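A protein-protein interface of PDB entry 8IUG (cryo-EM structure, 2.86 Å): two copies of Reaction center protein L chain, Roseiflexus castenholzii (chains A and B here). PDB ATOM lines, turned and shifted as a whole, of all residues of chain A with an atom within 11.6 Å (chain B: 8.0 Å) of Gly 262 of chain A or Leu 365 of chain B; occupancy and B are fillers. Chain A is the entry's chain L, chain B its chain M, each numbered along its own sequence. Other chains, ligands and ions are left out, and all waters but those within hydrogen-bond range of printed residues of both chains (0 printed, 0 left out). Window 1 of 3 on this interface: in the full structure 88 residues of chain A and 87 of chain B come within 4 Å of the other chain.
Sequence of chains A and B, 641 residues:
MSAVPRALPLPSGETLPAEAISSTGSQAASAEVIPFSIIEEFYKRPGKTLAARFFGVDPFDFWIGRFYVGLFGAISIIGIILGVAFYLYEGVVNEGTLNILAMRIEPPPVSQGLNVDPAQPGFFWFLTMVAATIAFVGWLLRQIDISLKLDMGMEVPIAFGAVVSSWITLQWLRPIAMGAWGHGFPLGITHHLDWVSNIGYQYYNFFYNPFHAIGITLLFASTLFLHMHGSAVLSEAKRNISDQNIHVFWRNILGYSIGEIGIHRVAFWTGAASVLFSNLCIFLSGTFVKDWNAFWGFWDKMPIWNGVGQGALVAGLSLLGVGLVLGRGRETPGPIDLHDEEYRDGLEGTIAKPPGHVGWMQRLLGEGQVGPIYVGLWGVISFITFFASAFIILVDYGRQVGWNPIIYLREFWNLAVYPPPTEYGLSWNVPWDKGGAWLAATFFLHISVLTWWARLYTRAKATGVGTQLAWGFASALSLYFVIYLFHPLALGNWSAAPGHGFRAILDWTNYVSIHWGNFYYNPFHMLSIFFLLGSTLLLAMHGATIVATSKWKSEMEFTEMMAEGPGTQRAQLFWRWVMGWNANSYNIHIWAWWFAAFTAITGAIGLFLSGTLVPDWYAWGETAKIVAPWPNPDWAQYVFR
No position is printed for both chains. Of the 11 pairs that touch across the chains among the printed residues, none has its exchanged pair printed and touching as well.
Printed residues of chain B within 4 Å of Ser 257 of chain A: Glu 367 (3.2 Å). Printed residues of chain B within 4 Å of Ile 258 of chain A: Leu 365 (3.7 Å) and Glu 367 (3.1 Å). Gly 262 of chain A touches just one residue of chain B: Leu 365. Ile 263 of chain A touches none of the printed residues of chain B. Of the printed residues of chain B, Arg 265 of chain A touches Leu 364 (2.5 Å) and Val 547 (3.96 Å). Of the printed residues of chain B, Trp 269 of chain A touches Leu 364 (3.8 Å). No residue of chain A comes within 4 Å of Gln 362 of chain B. Of the printed residues of chain A, Leu 364 of chain B touches Arg 265 and Trp 269. Printed residues of chain A within 4 Å of Leu 365 of chain B: Tyr 256, Ile 258 and Gly 262. Printed residues of chain A within 4 Å of Val 547 of chain B: Arg 265 (3.96 Å). The nearest printed residue of chain A that does not touch Leu 365 of chain B is Val 266 of chain A (4.02 Å).
Of the 23 printed residues of chain A, 8 touch a printed residue of chain B. Hydrophobic or aromatic side chains of chain A within 4 Å of the printed part of chain B: Tyr 256, Ile 261 and Trp 269. Printed residues of chain B that touch a printed residue of chain A: Leu 364, Leu 365, Glu 367, Val 547 and Glu 555. Hydrophobic or aromatic side chains of chain B that line the printed part of chain A: Leu 364, Leu 365 and Val 547. Among the printed residues, no Asp or Glu carboxylate lies within 4 Å of a Lys or Arg side-chain nitrogen of the other chain.
The side-chain hydroxyl (OH) of Tyr 256 of chain A is in hydrogen-bond range of the backbone carbonyl oxygen (O) of Glu 367 of chain B, at 2.9 Å. OE1 of Glu 367 of chain B sits close to O of Ser 257 of chain A, 3.2 Å away. The guanidinium group (NH1) of Arg 265 of chain A sits at hydrogen-bond distance from the backbone carbonyl oxygen (O) of Leu 364 of chain B, at 2.5 Å.
Tyr 256 of chain A touches Leu 365 of chain B. Ile 258 of chain A touches Leu 365 of chain B (O to O, 3.7 Å). Ile 258 of chain A touches Glu 367 of chain B (O to CB, 3.1 Å). Glu 260 of chain A touches Glu 555 of chain B (CB to O, 3.6 Å). Glu 555 of chain B touches Ile 261 of chain A (CG to N, 3.8 Å). Leu 365 of chain B touches Gly 262 of chain A (O to CA, 3.3 Å). Arg 265 of chain A touches Val 547 of chain B (CG to CG2, 3.96 Å). CH2 of Trp 269 of chain A touches CD2 of Leu 364 of chain B, at 3.8 Å.
A ring nitrogen (NE2) of His 247 of chain A sits at hydrogen-bond distance from the side-chain carboxylate (OE1) of Glu 260 of chain A, at 3.3 Å. A ring nitrogen (ND1) of His 264 of chain A lies within hydrogen-bond range of the backbone carbonyl oxygen of Glu 260 of chain A (2.9 Å).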
ATOM      1  N   PHE A 225     -12.244 -23.084  -1.813  1.00  0.00           N
ATOM      2  CA  PHE A 225     -12.424 -22.820  -3.240  1.00  0.00           C
ATOM      3  C   PHE A 225     -11.661 -21.579  -3.679  1.00  0.00           C
ATOM      4  O   PHE A 225     -11.114 -21.542  -4.785  1.00  0.00           O
ATOM      5  CB  PHE A 225     -13.907 -22.657  -3.574  1.00  0.00           C
ATOM      6  CG  PHE A 225     -14.704 -23.923  -3.473  1.00  0.00           C
ATOM      7  CD1 PHE A 225     -14.104 -25.156  -3.631  1.00  0.00           C
ATOM      8  CD2 PHE A 225     -16.063 -23.874  -3.222  1.00  0.00           C
ATOM      9  CE1 PHE A 225     -14.843 -26.315  -3.536  1.00  0.00           C
ATOM     10  CE2 PHE A 225     -16.805 -25.033  -3.124  1.00  0.00           C
ATOM     11  CZ  PHE A 225     -16.193 -26.253  -3.280  1.00  0.00           C
ATOM     12  N   LEU A 226     -11.642 -20.538  -2.844  1.00  0.00           N
ATOM     13  CA  LEU A 226     -10.881 -19.341  -3.186  1.00  0.00           C
ATOM     14  C   LEU A 226      -9.396 -19.648  -3.307  1.00  0.00           C
ATOM     15  O   LEU A 226      -8.739 -19.211  -4.260  1.00  0.00           O
ATOM     16  CB  LEU A 226     -11.115 -18.253  -2.140  1.00  0.00           C
ATOM     17  CG  LEU A 226     -10.468 -16.897  -2.413  1.00  0.00           C
ATOM     18  CD1 LEU A 226     -11.228 -16.123  -3.470  1.00  0.00           C
ATOM     19  CD2 LEU A 226     -10.350 -16.094  -1.147  1.00  0.00           C
ATOM     20  N   MET A 228      -8.053 -22.566  -4.017  1.00  0.00           N
ATOM     21  CA  MET A 228      -7.862 -23.418  -5.190  1.00  0.00           C
ATOM     22  C   MET A 228      -7.887 -22.613  -6.485  1.00  0.00           C
ATOM     23  O   MET A 228      -7.028 -22.795  -7.354  1.00  0.00           O
ATOM     24  CB  MET A 228      -8.929 -24.513  -5.214  1.00  0.00           C
ATOM     25  CG  MET A 228      -8.723 -25.616  -4.190  1.00  0.00           C
ATOM     26  SD  MET A 228      -9.975 -26.905  -4.274  1.00  0.00           S
ATOM     27  CE  MET A 228     -10.729 -26.567  -5.853  1.00  0.00           C
ATOM     28  N   HIS A 229      -8.868 -21.716  -6.637  1.00  0.00           N
ATOM     29  CA  HIS A 229      -8.961 -20.914  -7.854  1.00  0.00           C
ATOM     30  C   HIS A 229      -7.777 -19.965  -7.993  1.00  0.00           C
ATOM     31  O   HIS A 229      -7.228 -19.808  -9.093  1.00  0.00           O
ATOM     32  CB  HIS A 229     -10.274 -20.132  -7.875  1.00  0.00           C
ATOM     33  CG  HIS A 229     -10.461 -19.287  -9.102  1.00  0.00           C
ATOM     34  ND1 HIS A 229     -10.525 -19.817 -10.371  1.00  0.00           N
ATOM     35  CD2 HIS A 229     -10.598 -17.949  -9.250  1.00  0.00           C
ATOM     36  CE1 HIS A 229     -10.694 -18.844 -11.247  1.00  0.00           C
ATOM     37  NE2 HIS A 229     -10.741 -17.698 -10.593  1.00  0.00           N
ATOM     38  N   VAL A 233      -5.199 -20.208 -11.241  1.00  0.00           N
ATOM     39  CA  VAL A 233      -4.995 -19.158 -12.232  1.00  0.00           C
ATOM     40  C   VAL A 233      -3.568 -18.625 -12.173  1.00  0.00           C
ATOM     41  O   VAL A 233      -2.976 -18.302 -13.207  1.00  0.00           O
ATOM     42  CB  VAL A 233      -6.039 -18.043 -12.070  1.00  0.00           C
ATOM     43  CG1 VAL A 233      -5.829 -16.979 -13.125  1.00  0.00           C
ATOM     44  CG2 VAL A 233      -7.424 -18.620 -12.207  1.00  0.00           C
ATOM     45  N   HIS A 247      -6.769 -27.972 -17.314  1.00  0.00           N
ATOM     46  CA  HIS A 247      -7.784 -29.019 -17.290  1.00  0.00           C
ATOM     47  C   HIS A 247      -7.159 -30.388 -17.059  1.00  0.00           C
ATOM     48  O   HIS A 247      -7.674 -31.190 -16.273  1.00  0.00           O
ATOM     49  CB  HIS A 247      -8.580 -28.995 -18.590  1.00  0.00           C
ATOM     50  CG  HIS A 247      -9.331 -27.721 -18.809  1.00  0.00           C
ATOM     51  ND1 HIS A 247      -8.752 -26.599 -19.359  1.00  0.00           N
ATOM     52  CD2 HIS A 247     -10.613 -27.386 -18.539  1.00  0.00           C
ATOM     53  CE1 HIS A 247      -9.645 -25.630 -19.424  1.00  0.00           C
ATOM     54  NE2 HIS A 247     -10.784 -26.082 -18.932  1.00  0.00           N
ATOM     55  N   TRP A 250      -6.107 -30.550 -13.353  1.00  0.00           N
ATOM     56  CA  TRP A 250      -7.214 -30.783 -12.436  1.00  0.00           C
ATOM     57  C   TRP A 250      -7.948 -32.084 -12.700  1.00  0.00           C
ATOM     58  O   TRP A 250      -8.819 -32.446 -11.909  1.00  0.00           O
ATOM     59  CB  TRP A 250      -8.211 -29.626 -12.484  1.00  0.00           C
ATOM     60  CG  TRP A 250      -7.779 -28.431 -11.706  1.00  0.00           C
ATOM     61  CD1 TRP A 250      -7.402 -27.227 -12.206  1.00  0.00           C
ATOM     62  CD2 TRP A 250      -7.675 -28.326 -10.284  1.00  0.00           C
ATOM     63  NE1 TRP A 250      -7.069 -26.375 -11.188  1.00  0.00           N
ATOM     64  CE2 TRP A 250      -7.227 -27.028  -9.996  1.00  0.00           C
ATOM     65  CE3 TRP A 250      -7.914 -29.205  -9.227  1.00  0.00           C
ATOM     66  CZ2 TRP A 250      -7.018 -26.585  -8.697  1.00  0.00           C
ATOM     67  CZ3 TRP A 250      -7.710 -28.763  -7.940  1.00  0.00           C
ATOM     68  CH2 TRP A 250      -7.265 -27.468  -7.685  1.00  0.00           C
ATOM     69  N   TYR A 256     -11.740 -35.015 -11.993  1.00  0.00           N
ATOM     70  CA  TYR A 256     -12.773 -34.172 -12.586  1.00  0.00           C
ATOM     71  C   TYR A 256     -12.292 -32.733 -12.612  1.00  0.00           C
ATOM     72  O   TYR A 256     -11.782 -32.230 -11.610  1.00  0.00           O
ATOM     73  CB  TYR A 256     -14.093 -34.275 -11.810  1.00  0.00           C
ATOM     74  CG  TYR A 256     -15.164 -33.311 -12.278  1.00  0.00           C
ATOM     75  CD1 TYR A 256     -15.701 -33.407 -13.550  1.00  0.00           C
ATOM     76  CD2 TYR A 256     -15.643 -32.313 -11.443  1.00  0.00           C
ATOM     77  CE1 TYR A 256     -16.673 -32.534 -13.982  1.00  0.00           C
ATOM     78  CE2 TYR A 256     -16.616 -31.434 -11.867  1.00  0.00           C
ATOM     79  CZ  TYR A 256     -17.129 -31.550 -13.137  1.00  0.00           C
ATOM     80  OH  TYR A 256     -18.102 -30.681 -13.568  1.00  0.00           O
ATOM     81  N   SER A 257     -12.450 -32.031 -13.750  1.00  0.00           N
ATOM     82  CA  SER A 257     -12.162 -30.572 -13.897  1.00  0.00           C
ATOM     83  C   SER A 257     -13.478 -29.824 -14.162  1.00  0.00           C
ATOM     84  O   SER A 257     -14.138 -30.195 -15.134  1.00  0.00           O
ATOM     85  CB  SER A 257     -11.197 -30.318 -15.006  1.00  0.00           C
ATOM     86  OG  SER A 257     -10.963 -28.933 -15.172  1.00  0.00           O
ATOM     87  N   ILE A 258     -13.832 -28.786 -13.397  1.00  0.00           N
ATOM     88  CA  ILE A 258     -15.171 -28.108 -13.488  1.00  0.00           C
ATOM     89  C   ILE A 258     -15.363 -27.224 -14.729  1.00  0.00           C
ATOM     90  O   ILE A 258     -16.475 -27.215 -15.249  1.00  0.00           O
ATOM     91  CB  ILE A 258     -15.504 -27.324 -12.188  1.00  0.00           C
ATOM     92  CG1 ILE A 258     -16.971 -26.897 -12.112  1.00  0.00           C
ATOM     93  CG2 ILE A 258     -14.576 -26.141 -11.959  1.00  0.00           C
ATOM     94  CD1 ILE A 258     -17.456 -26.683 -10.710  1.00  0.00           C
ATOM     95  N   GLY A 259     -14.372 -26.451 -15.147  1.00  0.00           N
ATOM     96  CA  GLY A 259     -14.553 -25.507 -16.257  1.00  0.00           C
ATOM     97  C   GLY A 259     -14.221 -24.090 -15.852  1.00  0.00           C
ATOM     98  O   GLY A 259     -13.784 -23.898 -14.724  1.00  0.00           O
ATOM     99  N   GLU A 260     -14.462 -23.120 -16.729  1.00  0.00           N
ATOM    100  CA  GLU A 260     -14.080 -21.708 -16.481  1.00  0.00           C
ATOM    101  C   GLU A 260     -15.264 -20.877 -15.974  1.00  0.00           C
ATOM    102  O   GLU A 260     -15.044 -20.086 -15.077  1.00  0.00           O
ATOM    103  CB  GLU A 260     -13.453 -21.153 -17.756  1.00  0.00           C
ATOM    104  CG  GLU A 260     -11.962 -21.377 -17.837  1.00  0.00           C
ATOM    105  CD  GLU A 260     -11.534 -22.342 -18.925  1.00  0.00           C
ATOM    106  OE1 GLU A 260     -12.355 -23.197 -19.309  1.00  0.00           O
ATOM    107  OE2 GLU A 260     -10.382 -22.234 -19.391  1.00  0.00           O
ATOM    108  N   ILE A 261     -16.468 -21.030 -16.510  1.00  0.00           N
ATOM    109  CA  ILE A 261     -17.599 -20.306 -15.948  1.00  0.00           C
ATOM    110  C   ILE A 261     -18.165 -21.057 -14.747  1.00  0.00           C
ATOM    111  O   ILE A 261     -18.759 -20.446 -13.847  1.00  0.00           O
ATOM    112  CB  ILE A 261     -18.662 -20.070 -17.038  1.00  0.00           C
ATOM    113  CG1 ILE A 261     -19.797 -19.180 -16.525  1.00  0.00           C
ATOM    114  CG2 ILE A 261     -19.198 -21.390 -17.558  1.00  0.00           C
ATOM    115  CD1 ILE A 261     -19.368 -17.787 -16.137  1.00  0.00           C
ATOM    116  N   GLY A 262     -17.970 -22.376 -14.699  1.00  0.00           N
ATOM    117  CA  GLY A 262     -18.519 -23.163 -13.610  1.00  0.00           C
ATOM    118  C   GLY A 262     -17.897 -22.843 -12.267  1.00  0.00           C
ATOM    119  O   GLY A 262     -18.587 -22.821 -11.247  1.00  0.00           O
ATOM    120  N   ILE A 263     -16.591 -22.581 -12.242  1.00  0.00           N
ATOM    121  CA  ILE A 263     -15.937 -22.278 -10.974  1.00  0.00           C
ATOM    122  C   ILE A 263     -16.404 -20.930 -10.437  1.00  0.00           C
ATOM    123  O   ILE A 263     -16.628 -20.771  -9.232  1.00  0.00           O
ATOM    124  CB  ILE A 263     -14.404 -22.346 -11.121  1.00  0.00           C
ATOM    125  CG1 ILE A 263     -13.723 -22.054  -9.783  1.00  0.00           C
ATOM    126  CG2 ILE A 263     -13.905 -21.409 -12.200  1.00  0.00           C
ATOM    127  CD1 ILE A 263     -14.014 -23.074  -8.704  1.00  0.00           C
ATOM    128  N   HIS A 264     -16.587 -19.946 -11.316  1.00  0.00           N
ATOM    129  CA  HIS A 264     -17.043 -18.638 -10.860  1.00  0.00           C
ATOM    130  C   HIS A 264     -18.510 -18.689 -10.423  1.00  0.00           C
ATOM    131  O   HIS A 264     -18.895 -18.040  -9.438  1.00  0.00           O
ATOM    132  CB  HIS A 264     -16.784 -17.592 -11.954  1.00  0.00           C
ATOM    133  CG  HIS A 264     -15.322 -17.308 -12.203  1.00  0.00           C
ATOM    134  ND1 HIS A 264     -14.650 -17.775 -13.309  1.00  0.00           N
ATOM    135  CD2 HIS A 264     -14.412 -16.599 -11.488  1.00  0.00           C
ATOM    136  CE1 HIS A 264     -13.391 -17.372 -13.267  1.00  0.00           C
ATOM    137  NE2 HIS A 264     -13.215 -16.657 -12.169  1.00  0.00           N
ATOM    138  N   ARG A 265     -19.330 -19.505 -11.096  1.00  0.00           N
ATOM    139  CA  ARG A 265     -20.700 -19.737 -10.634  1.00  0.00           C
ATOM    140  C   ARG A 265     -20.725 -20.390  -9.257  1.00  0.00           C
ATOM    141  O   ARG A 265     -21.511 -20.001  -8.386  1.00  0.00           O
ATOM    142  CB  ARG A 265     -21.455 -20.620 -11.625  1.00  0.00           C
ATOM    143  CG  ARG A 265     -21.829 -19.976 -12.928  1.00  0.00           C
ATOM    144  CD  ARG A 265     -22.521 -20.984 -13.814  1.00  0.00           C
ATOM    145  NE  ARG A 265     -22.753 -20.475 -15.158  1.00  0.00           N
ATOM    146  CZ  ARG A 265     -23.175 -21.216 -16.173  1.00  0.00           C
ATOM    147  NH1 ARG A 265     -23.424 -22.504 -16.027  1.00  0.00           N
ATOM    148  NH2 ARG A 265     -23.346 -20.650 -17.362  1.00  0.00           N
ATOM    149  N   VAL A 266     -19.897 -21.417  -9.058  1.00  0.00           N
ATOM    150  CA  VAL A 266     -19.839 -22.105  -7.770  1.00  0.00           C
ATOM    151  C   VAL A 266     -19.407 -21.143  -6.673  1.00  0.00           C
ATOM    152  O   VAL A 266     -19.950 -21.158  -5.562  1.00  0.00           O
ATOM    153  CB  VAL A 266     -18.902 -23.325  -7.867  1.00  0.00           C
ATOM    154  CG1 VAL A 266     -18.479 -23.801  -6.493  1.00  0.00           C
ATOM    155  CG2 VAL A 266     -19.580 -24.448  -8.622  1.00  0.00           C
ATOM    156  N   ALA A 267     -18.425 -20.289  -6.972  1.00  0.00           N
ATOM    157  CA  ALA A 267     -17.991 -19.268  -6.025  1.00  0.00           C
ATOM    158  C   ALA A 267     -19.146 -18.372  -5.601  1.00  0.00           C
ATOM    159  O   ALA A 267     -19.410 -18.191  -4.405  1.00  0.00           O
ATOM    160  CB  ALA A 267     -16.880 -18.436  -6.659  1.00  0.00           C
ATOM    161  N   PHE A 268     -19.853 -17.808  -6.582  1.00  0.00           N
ATOM    162  CA  PHE A 268     -20.984 -16.929  -6.300  1.00  0.00           C
ATOM    163  C   PHE A 268     -22.037 -17.630  -5.437  1.00  0.00           C
ATOM    164  O   PHE A 268     -22.456 -17.109  -4.388  1.00  0.00           O
ATOM    165  CB  PHE A 268     -21.553 -16.454  -7.642  1.00  0.00           C
ATOM    166  CG  PHE A 268     -22.873 -15.752  -7.560  1.00  0.00           C
ATOM    167  CD1 PHE A 268     -23.147 -14.845  -6.555  1.00  0.00           C
ATOM    168  CD2 PHE A 268     -23.827 -15.967  -8.535  1.00  0.00           C
ATOM    169  CE1 PHE A 268     -24.359 -14.203  -6.507  1.00  0.00           C
ATOM    170  CE2 PHE A 268     -25.037 -15.323  -8.488  1.00  0.00           C
ATOM    171  CZ  PHE A 268     -25.303 -14.442  -7.476  1.00  0.00           C
ATOM    172  N   TRP A 269     -22.451 -18.830  -5.852  1.00  0.00           N
ATOM    173  CA  TRP A 269     -23.541 -19.523  -5.173  1.00  0.00           C
ATOM    174  C   TRP A 269     -23.166 -19.894  -3.741  1.00  0.00           C
ATOM    175  O   TRP A 269     -23.957 -19.697  -2.810  1.00  0.00           O
ATOM    176  CB  TRP A 269     -23.938 -20.767  -5.969  1.00  0.00           C
ATOM    177  CG  TRP A 269     -24.600 -20.472  -7.284  1.00  0.00           C
ATOM    178  CD1 TRP A 269     -25.241 -19.328  -7.636  1.00  0.00           C
ATOM    179  CD2 TRP A 269     -24.683 -21.342  -8.420  1.00  0.00           C
ATOM    180  NE1 TRP A 269     -25.718 -19.424  -8.917  1.00  0.00           N
ATOM    181  CE2 TRP A 269     -25.388 -20.653  -9.421  1.00  0.00           C
ATOM    182  CE3 TRP A 269     -24.226 -22.634  -8.688  1.00  0.00           C
ATOM    183  CZ2 TRP A 269     -25.648 -21.211 -10.665  1.00  0.00           C
ATOM    184  CZ3 TRP A 269     -24.487 -23.182  -9.924  1.00  0.00           C
ATOM    185  CH2 TRP A 269     -25.190 -22.474 -10.896  1.00  0.00           C
ATOM    186  N   THR A 270     -21.961 -20.441  -3.546  1.00  0.00           N
ATOM    187  CA  THR A 270     -21.528 -20.832  -2.206  1.00  0.00           C
ATOM    188  C   THR A 270     -21.413 -19.623  -1.287  1.00  0.00           C
ATOM    189  O   THR A 270     -21.856 -19.666  -0.127  1.00  0.00           O
ATOM    190  CB  THR A 270     -20.190 -21.566  -2.289  1.00  0.00           C
ATOM    191  OG1 THR A 270     -20.220 -22.483  -3.387  1.00  0.00           O
ATOM    192  CG2 THR A 270     -19.924 -22.336  -1.018  1.00  0.00           C
ATOM    193  N   GLY A 271     -20.831 -18.529  -1.792  1.00  0.00           N
ATOM    194  CA  GLY A 271     -20.721 -17.329  -0.985  1.00  0.00           C
ATOM    195  C   GLY A 271     -22.062 -16.824  -0.496  1.00  0.00           C
ATOM    196  O   GLY A 271     -22.216 -16.496   0.681  1.00  0.00           O
ATOM    197  N   GLY B 359     -24.943 -35.482 -17.162  1.00  0.00           N
ATOM    198  CA  GLY B 359     -25.730 -34.459 -17.827  1.00  0.00           C
ATOM    199  C   GLY B 359     -26.046 -33.218 -17.019  1.00  0.00           C
ATOM    200  O   GLY B 359     -25.951 -32.101 -17.537  1.00  0.00           O
ATOM    201  N   TRP B 360     -26.439 -33.389 -15.756  1.00  0.00           N
ATOM    202  CA  TRP B 360     -26.804 -32.228 -14.953  1.00  0.00           C
ATOM    203  C   TRP B 360     -25.591 -31.369 -14.634  1.00  0.00           C
ATOM    204  O   TRP B 360     -25.714 -30.144 -14.523  1.00  0.00           O
ATOM    205  CB  TRP B 360     -27.520 -32.663 -13.671  1.00  0.00           C
ATOM    206  CG  TRP B 360     -26.668 -33.363 -12.655  1.00  0.00           C
ATOM    207  CD1 TRP B 360     -26.494 -34.704 -12.522  1.00  0.00           C
ATOM    208  CD2 TRP B 360     -25.897 -32.754 -11.612  1.00  0.00           C
ATOM    209  NE1 TRP B 360     -25.654 -34.972 -11.473  1.00  0.00           N
ATOM    210  CE2 TRP B 360     -25.274 -33.790 -10.897  1.00  0.00           C
ATOM    211  CE3 TRP B 360     -25.666 -31.433 -11.221  1.00  0.00           C
ATOM    212  CZ2 TRP B 360     -24.436 -33.547  -9.814  1.00  0.00           C
ATOM    213  CZ3 TRP B 360     -24.834 -31.195 -10.148  1.00  0.00           C
ATOM    214  CH2 TRP B 360     -24.230 -32.245  -9.457  1.00  0.00           C
ATOM    215  N   MET B 361     -24.414 -31.984 -14.498  1.00  0.00           N
ATOM    216  CA  MET B 361     -23.187 -31.210 -14.364  1.00  0.00           C
ATOM    217  C   MET B 361     -22.896 -30.431 -15.637  1.00  0.00           C
ATOM    218  O   MET B 361     -22.426 -29.293 -15.580  1.00  0.00           O
ATOM    219  CB  MET B 361     -22.019 -32.131 -14.019  1.00  0.00           C
ATOM    220  CG  MET B 361     -22.124 -32.769 -12.650  1.00  0.00           C
ATOM    221  SD  MET B 361     -20.654 -33.684 -12.166  1.00  0.00           S
ATOM    222  CE  MET B 361     -20.221 -32.834 -10.657  1.00  0.00           C
ATOM    223  N   GLN B 362     -23.182 -31.024 -16.796  1.00  0.00           N
ATOM    224  CA  GLN B 362     -23.002 -30.310 -18.055  1.00  0.00           C
ATOM    225  C   GLN B 362     -23.934 -29.111 -18.149  1.00  0.00           C
ATOM    226  O   GLN B 362     -23.538 -28.044 -18.630  1.00  0.00           O
ATOM    227  CB  GLN B 362     -23.229 -31.257 -19.231  1.00  0.00           C
ATOM    228  CG  GLN B 362     -22.985 -30.636 -20.592  1.00  0.00           C
ATOM    229  CD  GLN B 362     -21.516 -30.521 -20.930  1.00  0.00           C
ATOM    230  OE1 GLN B 362     -20.675 -31.152 -20.299  1.00  0.00           O
ATOM    231  NE2 GLN B 362     -21.201 -29.715 -21.931  1.00  0.00           N
ATOM    232  N   ARG B 363     -25.183 -29.267 -17.704  1.00  0.00           N
ATOM    233  CA  ARG B 363     -26.136 -28.164 -17.804  1.00  0.00           C
ATOM    234  C   ARG B 363     -25.837 -27.060 -16.797  1.00  0.00           C
ATOM    235  O   ARG B 363     -25.882 -25.874 -17.143  1.00  0.00           O
ATOM    236  CB  ARG B 363     -27.560 -28.675 -17.623  1.00  0.00           C
ATOM    237  CG  ARG B 363     -28.087 -29.447 -18.807  1.00  0.00           C
ATOM    238  CD  ARG B 363     -29.601 -29.501 -18.793  1.00  0.00           C
ATOM    239  NE  ARG B 363     -30.199 -28.182 -18.961  1.00  0.00           N
ATOM    240  CZ  ARG B 363     -31.489 -27.973 -19.182  1.00  0.00           C
ATOM    241  NH1 ARG B 363     -32.345 -28.974 -19.270  1.00  0.00           N
ATOM    242  NH2 ARG B 363     -31.929 -26.727 -19.323  1.00  0.00           N
ATOM    243  N   LEU B 364     -25.544 -27.416 -15.546  1.00  0.00           N
ATOM    244  CA  LEU B 364     -25.316 -26.399 -14.523  1.00  0.00           C
ATOM    245  C   LEU B 364     -23.905 -25.831 -14.605  1.00  0.00           C
ATOM    246  O   LEU B 364     -23.717 -24.627 -14.807  1.00  0.00           O
ATOM    247  CB  LEU B 364     -25.557 -26.984 -13.132  1.00  0.00           C
ATOM    248  CG  LEU B 364     -26.831 -26.640 -12.362  1.00  0.00           C
ATOM    249  CD1 LEU B 364     -26.623 -26.959 -10.896  1.00  0.00           C
ATOM    250  CD2 LEU B 364     -27.230 -25.190 -12.544  1.00  0.00           C
ATOM    251  N   LEU B 365     -22.901 -26.688 -14.441  1.00  0.00           N
ATOM    252  CA  LEU B 365     -21.523 -26.253 -14.281  1.00  0.00           C
ATOM    253  C   LEU B 365     -20.798 -26.049 -15.603  1.00  0.00           C
ATOM    254  O   LEU B 365     -19.718 -25.454 -15.607  1.00  0.00           O
ATOM    255  CB  LEU B 365     -20.776 -27.272 -13.420  1.00  0.00           C
ATOM    256  CG  LEU B 365     -21.568 -27.693 -12.177  1.00  0.00           C
ATOM    257  CD1 LEU B 365     -20.885 -28.817 -11.428  1.00  0.00           C
ATOM    258  CD2 LEU B 365     -21.800 -26.503 -11.264  1.00  0.00           C
ATOM    259  N   GLY B 366     -21.356 -26.517 -16.718  1.00  0.00           N
ATOM    260  CA  GLY B 366     -20.753 -26.315 -18.015  1.00  0.00           C
ATOM    261  C   GLY B 366     -19.787 -27.389 -18.468  1.00  0.00           C
ATOM    262  O   GLY B 366     -19.296 -27.311 -19.598  1.00  0.00           O
ATOM    263  N   GLU B 367     -19.498 -28.381 -17.631  1.00  0.00           N
ATOM    264  CA  GLU B 367     -18.594 -29.463 -17.993  1.00  0.00           C
ATOM    265  C   GLU B 367     -19.047 -30.732 -17.289  1.00  0.00           C
ATOM    266  O   GLU B 367     -19.417 -30.691 -16.115  1.00  0.00           O
ATOM    267  CB  GLU B 367     -17.149 -29.136 -17.612  1.00  0.00           C
ATOM    268  CG  GLU B 367     -16.143 -29.427 -18.697  1.00  0.00           C
ATOM    269  CD  GLU B 367     -15.842 -30.904 -18.825  1.00  0.00           C
ATOM    270  OE1 GLU B 367     -15.346 -31.496 -17.844  1.00  0.00           O
ATOM    271  OE2 GLU B 367     -16.103 -31.474 -19.905  1.00  0.00           O
ATOM    272  N   GLY B 368     -19.006 -31.857 -18.001  1.00  0.00           N
ATOM    273  CA  GLY B 368     -19.550 -33.086 -17.458  1.00  0.00           C
ATOM    274  C   GLY B 368     -18.687 -34.325 -17.572  1.00  0.00           C
ATOM    275  O   GLY B 368     -19.079 -35.387 -17.089  1.00  0.00           O
ATOM    276  N   VAL B 547     -19.554 -13.660 -13.516  1.00  0.00           N
ATOM    277  CA  VAL B 547     -20.781 -14.171 -14.121  1.00  0.00           C
ATOM    278  C   VAL B 547     -21.592 -13.038 -14.743  1.00  0.00           C
ATOM    279  O   VAL B 547     -22.227 -13.216 -15.789  1.00  0.00           O
ATOM    280  CB  VAL B 547     -21.600 -14.963 -13.087  1.00  0.00           C
ATOM    281  CG1 VAL B 547     -22.905 -15.417 -13.683  1.00  0.00           C
ATOM    282  CG2 VAL B 547     -20.818 -16.157 -12.621  1.00  0.00           C
ATOM    283  N   GLU B 555     -14.767 -14.950 -18.545  1.00  0.00           N
ATOM    284  CA  GLU B 555     -14.298 -16.043 -17.704  1.00  0.00           C
ATOM    285  C   GLU B 555     -13.123 -16.790 -18.310  1.00  0.00           C
ATOM    286  O   GLU B 555     -12.562 -17.668 -17.649  1.00  0.00           O
ATOM    287  CB  GLU B 555     -15.434 -17.026 -17.429  1.00  0.00           C
ATOM    288  CG  GLU B 555     -15.815 -17.888 -18.614  1.00  0.00           C
ATOM    289  CD  GLU B 555     -16.812 -17.222 -19.528  1.00  0.00           C
ATOM    290  OE1 GLU B 555     -17.318 -16.145 -19.167  1.00  0.00           O
ATOM    291  OE2 GLU B 555     -17.097 -17.779 -20.605  1.00  0.00           O
